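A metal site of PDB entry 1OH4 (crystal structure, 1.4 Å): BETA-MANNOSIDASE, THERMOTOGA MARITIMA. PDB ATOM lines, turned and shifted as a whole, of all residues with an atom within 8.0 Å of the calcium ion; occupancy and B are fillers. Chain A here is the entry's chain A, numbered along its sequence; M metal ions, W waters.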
ATOM      1  N   VAL A  14      -9.359  -8.605  -2.562  1.00  0.00           N
ATOM      2  CA  VAL A  14      -9.367  -7.161  -2.652  1.00  0.00           C
ATOM      3  C   VAL A  14     -10.712  -6.691  -2.067  1.00  0.00           C
ATOM      4  O   VAL A  14     -11.777  -6.994  -2.597  1.00  0.00           O
ATOM      5  CB  VAL A  14      -9.196  -6.677  -4.094  1.00  0.00           C
ATOM      6  CG1 VAL A  14      -9.316  -5.182  -4.153  1.00  0.00           C
ATOM      7  CG2 VAL A  14      -7.859  -7.138  -4.672  1.00  0.00           C
ATOM      8  N   ASP A  15     -10.645  -5.975  -0.962  1.00  0.00           N
ATOM      9  CA  ASP A  15     -11.814  -5.384  -0.301  1.00  0.00           C
ATOM     10  C   ASP A  15     -11.921  -3.871  -0.472  1.00  0.00           C
ATOM     11  O   ASP A  15     -12.873  -3.279   0.010  1.00  0.00           O
ATOM     12  CB  ASP A  15     -11.814  -5.733   1.184  1.00  0.00           C
ATOM     13  CG  ASP A  15     -11.940  -7.178   1.409  1.00  0.00           C
ATOM     14  OD1 ASP A  15     -12.611  -7.872   0.621  1.00  0.00           O
ATOM     15  OD2 ASP A  15     -11.385  -7.726   2.370  1.00  0.00           O
ATOM     16  N   PHE A  16     -10.983  -3.265  -1.150  1.00  0.00           N
ATOM     17  CA  PHE A  16     -11.014  -1.838  -1.460  1.00  0.00           C
ATOM     18  C   PHE A  16     -11.062  -0.925  -0.218  1.00  0.00           C
ATOM     19  O   PHE A  16     -11.818   0.009  -0.124  1.00  0.00           O
ATOM     20  CB  PHE A  16     -12.163  -1.504  -2.403  1.00  0.00           C
ATOM     21  CG  PHE A  16     -12.127  -2.285  -3.695  1.00  0.00           C
ATOM     22  CD1 PHE A  16     -11.295  -1.887  -4.754  1.00  0.00           C
ATOM     23  CD2 PHE A  16     -12.909  -3.396  -3.861  1.00  0.00           C
ATOM     24  CE1 PHE A  16     -11.232  -2.639  -5.929  1.00  0.00           C
ATOM     25  CE2 PHE A  16     -12.850  -4.141  -5.048  1.00  0.00           C
ATOM     26  CZ  PHE A  16     -11.998  -3.742  -6.072  1.00  0.00           C
ATOM     27  N   SER A  17     -10.188  -1.227   0.723  1.00  0.00           N
ATOM     28  CA  SER A  17      -9.993  -0.449   1.963  1.00  0.00           C
ATOM     29  C   SER A  17      -9.693   1.006   1.837  1.00  0.00           C
ATOM     30  O   SER A  17     -10.117   1.717   2.731  1.00  0.00           O
ATOM     31  CB  SER A  17      -8.843  -1.062   2.754  1.00  0.00           C
ATOM     32  OG  SER A  17      -9.211  -2.316   3.254  1.00  0.00           O
ATOM     33  N   SER A  18      -8.920   1.451   0.832  1.00  0.00           N
ATOM     34  CA  SER A  18      -8.601   2.890   0.557  1.00  0.00           C
ATOM     35  C   SER A  18      -8.456   3.202  -0.912  1.00  0.00           C
ATOM     36  O   SER A  18      -8.379   2.223  -1.738  1.00  0.00           O
ATOM     37  CB  SER A  18      -7.328   3.347   1.321  1.00  0.00           C
ATOM     38  OG  SER A  18      -6.151   3.041   0.587  1.00  0.00           O
ATOM     39  N   TRP A  42     -12.641   5.410  -6.110  1.00  0.00           N
ATOM     40  CA  TRP A  42     -12.957   4.813  -4.841  1.00  0.00           C
ATOM     41  C   TRP A  42     -14.221   5.422  -4.265  1.00  0.00           C
ATOM     42  O   TRP A  42     -14.509   6.609  -4.480  1.00  0.00           O
ATOM     43  CB  TRP A  42     -11.834   5.102  -3.843  1.00  0.00           C
ATOM     44  CG  TRP A  42     -11.901   4.332  -2.592  1.00  0.00           C
ATOM     45  CD1 TRP A  42     -11.777   2.988  -2.426  1.00  0.00           C
ATOM     46  CD2 TRP A  42     -12.112   4.863  -1.278  1.00  0.00           C
ATOM     47  NE1 TRP A  42     -11.878   2.643  -1.098  1.00  0.00           N
ATOM     48  CE2 TRP A  42     -12.067   3.790  -0.379  1.00  0.00           C
ATOM     49  CE3 TRP A  42     -12.302   6.155  -0.772  1.00  0.00           C
ATOM     50  CZ2 TRP A  42     -12.184   3.960   1.008  1.00  0.00           C
ATOM     51  CZ3 TRP A  42     -12.469   6.313   0.574  1.00  0.00           C
ATOM     52  CH2 TRP A  42     -12.412   5.229   1.447  1.00  0.00           C
ATOM     53  N   ASN A  43     -14.984   4.613  -3.545  1.00  0.00           N
ATOM     54  CA  ASN A  43     -16.115   5.076  -2.757  1.00  0.00           C
ATOM     55  C   ASN A  43     -15.952   4.542  -1.359  1.00  0.00           C
ATOM     56  O   ASN A  43     -15.822   3.329  -1.166  1.00  0.00           O
ATOM     57  CB  ASN A  43     -17.432   4.632  -3.357  1.00  0.00           C
ATOM     58  CG  ASN A  43     -18.629   5.203  -2.648  1.00  0.00           C
ATOM     59  OD1 ASN A  43     -18.917   4.872  -1.487  1.00  0.00           O
ATOM     60  ND2 ASN A  43     -19.374   6.039  -3.366  1.00  0.00           N
ATOM     61  N   GLY A  44     -15.959   5.443  -0.364  1.00  0.00           N
ATOM     62  CA  GLY A  44     -15.692   5.028   0.982  1.00  0.00           C
ATOM     63  C   GLY A  44     -16.931   4.704   1.787  1.00  0.00           C
ATOM     64  O   GLY A  44     -16.785   4.217   2.898  1.00  0.00           O
ATOM     65  N   GLU A  45     -18.126   4.893   1.232  1.00  0.00           N
ATOM     66  CA  GLU A  45     -19.335   4.496   1.970  1.00  0.00           C
ATOM     67  C   GLU A  45     -19.821   3.080   1.659  1.00  0.00           C
ATOM     68  O   GLU A  45     -20.126   2.216   2.518  1.00  0.00           O
ATOM     69  CB  GLU A  45     -20.444   5.513   1.738  1.00  0.00           C
ATOM     70  CG  GLU A  45     -21.641   5.279   2.645  1.00  0.00           C
ATOM     71  CD  GLU A  45     -21.625   6.164   3.885  1.00  0.00           C
ATOM     72  OE1 GLU A  45     -21.875   7.363   3.698  1.00  0.00           O
ATOM     73  OE2 GLU A  45     -21.366   5.650   5.003  1.00  0.00           O
ATOM     74  N   VAL A  46     -19.856   2.775   0.398  1.00  0.00           N
ATOM     75  CA  VAL A  46     -20.364   1.495  -0.017  1.00  0.00           C
ATOM     76  C   VAL A  46     -19.327   0.425   0.319  1.00  0.00           C
ATOM     77  O   VAL A  46     -18.148   0.573   0.016  1.00  0.00           O
ATOM     78  CB  VAL A  46     -20.609   1.529  -1.518  1.00  0.00           C
ATOM     79  CG1 VAL A  46     -21.018   0.163  -2.046  1.00  0.00           C
ATOM     80  CG2 VAL A  46     -21.659   2.566  -1.842  1.00  0.00           C
ATOM     81  N   GLY A  47     -19.774  -0.659   0.946  1.00  0.00           N
ATOM     82  CA  GLY A  47     -18.905  -1.801   1.222  1.00  0.00           C
ATOM     83  C   GLY A  47     -17.727  -1.455   2.132  1.00  0.00           C
ATOM     84  O   GLY A  47     -16.725  -2.165   2.139  1.00  0.00           O
ATOM     85  N   ASN A  48     -17.847  -0.373   2.937  1.00  0.00           N
ATOM     86  CA  ASN A  48     -16.714   0.124   3.727  1.00  0.00           C
ATOM     87  C   ASN A  48     -15.490   0.321   2.841  1.00  0.00           C
ATOM     88  O   ASN A  48     -14.370   0.040   3.235  1.00  0.00           O
ATOM     89  CB  ASN A  48     -16.395  -0.804   4.918  1.00  0.00           C
ATOM     90  CG  ASN A  48     -15.751  -0.052   6.064  1.00  0.00           C
ATOM     91  OD1 ASN A  48     -14.602  -0.283   6.418  1.00  0.00           O
ATOM     92  ND2 ASN A  48     -16.504   0.883   6.643  1.00  0.00           N
ATOM     93  N   GLY A  49     -15.730   0.809   1.627  1.00  0.00           N
ATOM     94  CA  GLY A  49     -14.707   0.908   0.594  1.00  0.00           C
ATOM     95  C   GLY A  49     -15.027  -0.017  -0.543  1.00  0.00           C
ATOM     96  O   GLY A  49     -15.144  -1.230  -0.353  1.00  0.00           O
ATOM     97  N   ALA A  50     -15.243   0.565  -1.722  1.00  0.00           N
ATOM     98  CA  ALA A  50     -15.624  -0.249  -2.896  1.00  0.00           C
ATOM     99  C   ALA A  50     -15.139   0.452  -4.129  1.00  0.00           C
ATOM    100  O   ALA A  50     -14.842   1.635  -4.100  1.00  0.00           O
ATOM    101  CB  ALA A  50     -17.114  -0.482  -2.981  1.00  0.00           C
ATOM    102  N   LEU A  51     -15.063  -0.294  -5.230  1.00  0.00           N
ATOM    103  CA  LEU A  51     -14.713   0.262  -6.507  1.00  0.00           C
ATOM    104  C   LEU A  51     -15.954   0.780  -7.194  1.00  0.00           C
ATOM    105  O   LEU A  51     -16.875   0.008  -7.440  1.00  0.00           O
ATOM    106  CB  LEU A  51     -14.035  -0.811  -7.354  1.00  0.00           C
ATOM    107  CG  LEU A  51     -13.383  -0.320  -8.639  1.00  0.00           C
ATOM    108  CD1 LEU A  51     -12.170   0.521  -8.366  1.00  0.00           C
ATOM    109  CD2 LEU A  51     -12.984  -1.522  -9.532  1.00  0.00           C
ATOM    110  N   TYR A  86     -22.905  -4.159  -6.499  1.00  0.00           N
ATOM    111  CA  TYR A  86     -23.980  -3.379  -5.850  1.00  0.00           C
ATOM    112  C   TYR A  86     -24.465  -2.316  -6.805  1.00  0.00           C
ATOM    113  O   TYR A  86     -23.672  -1.568  -7.367  1.00  0.00           O
ATOM    114  CB  TYR A  86     -23.499  -2.722  -4.543  1.00  0.00           C
ATOM    115  CG  TYR A  86     -22.842  -3.637  -3.547  1.00  0.00           C
ATOM    116  CD1 TYR A  86     -23.442  -4.801  -3.140  1.00  0.00           C
ATOM    117  CD2 TYR A  86     -21.626  -3.329  -3.005  1.00  0.00           C
ATOM    118  CE1 TYR A  86     -22.866  -5.636  -2.233  1.00  0.00           C
ATOM    119  CE2 TYR A  86     -21.022  -4.186  -2.069  1.00  0.00           C
ATOM    120  CZ  TYR A  86     -21.650  -5.329  -1.691  1.00  0.00           C
ATOM    121  OH  TYR A  86     -21.130  -6.211  -0.750  1.00  0.00           O
ATOM    122  N   PHE A 127     -26.011   0.290   3.133  1.00  0.00           N
ATOM    123  CA  PHE A 127     -24.776   0.975   3.532  1.00  0.00           C
ATOM    124  C   PHE A 127     -25.163   2.431   3.790  1.00  0.00           C
ATOM    125  O   PHE A 127     -25.704   3.093   2.911  1.00  0.00           O
ATOM    126  CB  PHE A 127     -23.691   0.897   2.441  1.00  0.00           C
ATOM    127  CG  PHE A 127     -23.203  -0.483   2.125  1.00  0.00           C
ATOM    128  CD1 PHE A 127     -22.488  -1.219   3.040  1.00  0.00           C
ATOM    129  CD2 PHE A 127     -23.434  -1.043   0.882  1.00  0.00           C
ATOM    130  CE1 PHE A 127     -22.030  -2.502   2.736  1.00  0.00           C
ATOM    131  CE2 PHE A 127     -22.990  -2.328   0.606  1.00  0.00           C
ATOM    132  CZ  PHE A 127     -22.299  -3.034   1.513  1.00  0.00           C
ATOM    133  N   ILE A 167     -18.194  -2.568  -7.284  1.00  0.00           N
ATOM    134  CA  ILE A 167     -17.596  -3.883  -7.140  1.00  0.00           C
ATOM    135  C   ILE A 167     -16.931  -3.979  -5.775  1.00  0.00           C
ATOM    136  O   ILE A 167     -16.280  -3.035  -5.330  1.00  0.00           O
ATOM    137  CB  ILE A 167     -16.564  -4.174  -8.279  1.00  0.00           C
ATOM    138  CG1 ILE A 167     -17.307  -4.239  -9.622  1.00  0.00           C
ATOM    139  CG2 ILE A 167     -15.760  -5.458  -8.001  1.00  0.00           C
ATOM    140  CD1 ILE A 167     -16.394  -4.182 -10.860  1.00  0.00           C
ATOM    141  N   ASP A 168     -17.067  -5.111  -5.125  1.00  0.00           N
ATOM    142  CA  ASP A 168     -16.392  -5.316  -3.848  1.00  0.00           C
ATOM    143  C   ASP A 168     -16.096  -6.807  -3.668  1.00  0.00           C
ATOM    144  O   ASP A 168     -16.625  -7.673  -4.353  1.00  0.00           O
ATOM    145  CB  ASP A 168     -17.277  -4.778  -2.706  1.00  0.00           C
ATOM    146  CG  ASP A 168     -16.513  -4.394  -1.448  1.00  0.00           C
ATOM    147  OD1 ASP A 168     -15.244  -4.488  -1.393  1.00  0.00           O
ATOM    148  OD2 ASP A 168     -17.119  -3.898  -0.486  1.00  0.00           O
ATOM    149  N   ASN A 169     -15.264  -7.098  -2.666  1.00  0.00           N
ATOM    150  CA  ASN A 169     -15.007  -8.458  -2.201  1.00  0.00           C
ATOM    151  C   ASN A 169     -14.555  -9.378  -3.302  1.00  0.00           C
ATOM    152  O   ASN A 169     -15.075 -10.456  -3.485  1.00  0.00           O
ATOM    153  CB  ASN A 169     -16.235  -9.035  -1.487  1.00  0.00           C
ATOM    154  CG  ASN A 169     -16.752  -8.096  -0.414  1.00  0.00           C
ATOM    155  OD1 ASN A 169     -15.970  -7.599   0.381  1.00  0.00           O
ATOM    156  ND2 ASN A 169     -18.057  -7.807  -0.417  1.00  0.00           N
ATOM    157  N   VAL A 170     -13.515  -8.951  -4.019  1.00  0.00           N
ATOM    158  CA  VAL A 170     -12.946  -9.781  -5.084  1.00  0.00           C
ATOM    159  C   VAL A 170     -12.064 -10.839  -4.423  1.00  0.00           C
ATOM    160  O   VAL A 170     -11.126 -10.485  -3.731  1.00  0.00           O
ATOM    161  CB  VAL A 170     -12.140  -8.918  -6.090  1.00  0.00           C
ATOM    162  CG1 VAL A 170     -11.507  -9.792  -7.166  1.00  0.00           C
ATOM    163  CG2 VAL A 170     -13.029  -7.841  -6.713  1.00  0.00           C
HETATM  164 CA    CA M   1     -15.117  -3.246   0.767  1.00  0.00          CA
HETATM  165  O   HOH W   1     -13.863  -2.710   2.745  1.00  0.00           O
HETATM  166  O   HOH W   2     -15.316  -5.356   1.818  1.00  0.00           O
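The side-chain carboxylate (OD1) of Asp 15 lies close to the side-chain amide oxygen (OD1) of Asn 169.
Of the 21 residues printed, 4 come within 4 Å of the calcium ion.
The nearest printed residue that does not touch the calcium ion is Asn 48 (4.1 Å).
The calcium ion is bound by O of Gly 49.
Water W2 is bound to the calcium ion (2.4 Å).
O of Asp 15 is bound to the calcium ion (2.4 Å).
The calcium ion is bound by O of Gly 47 (2.4 Å).
Water W1 is bound to the calcium ion (2.4 Å).
The calcium ion is bound by the side-chain carboxylate (OD2) of Asp 168, at 2.5 Å.
The calcium ion is bound by the side-chain carboxylate (OD1) of Asp 168, 2.5 Å away.
The calcium ion has seven donor atoms within binding distance.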
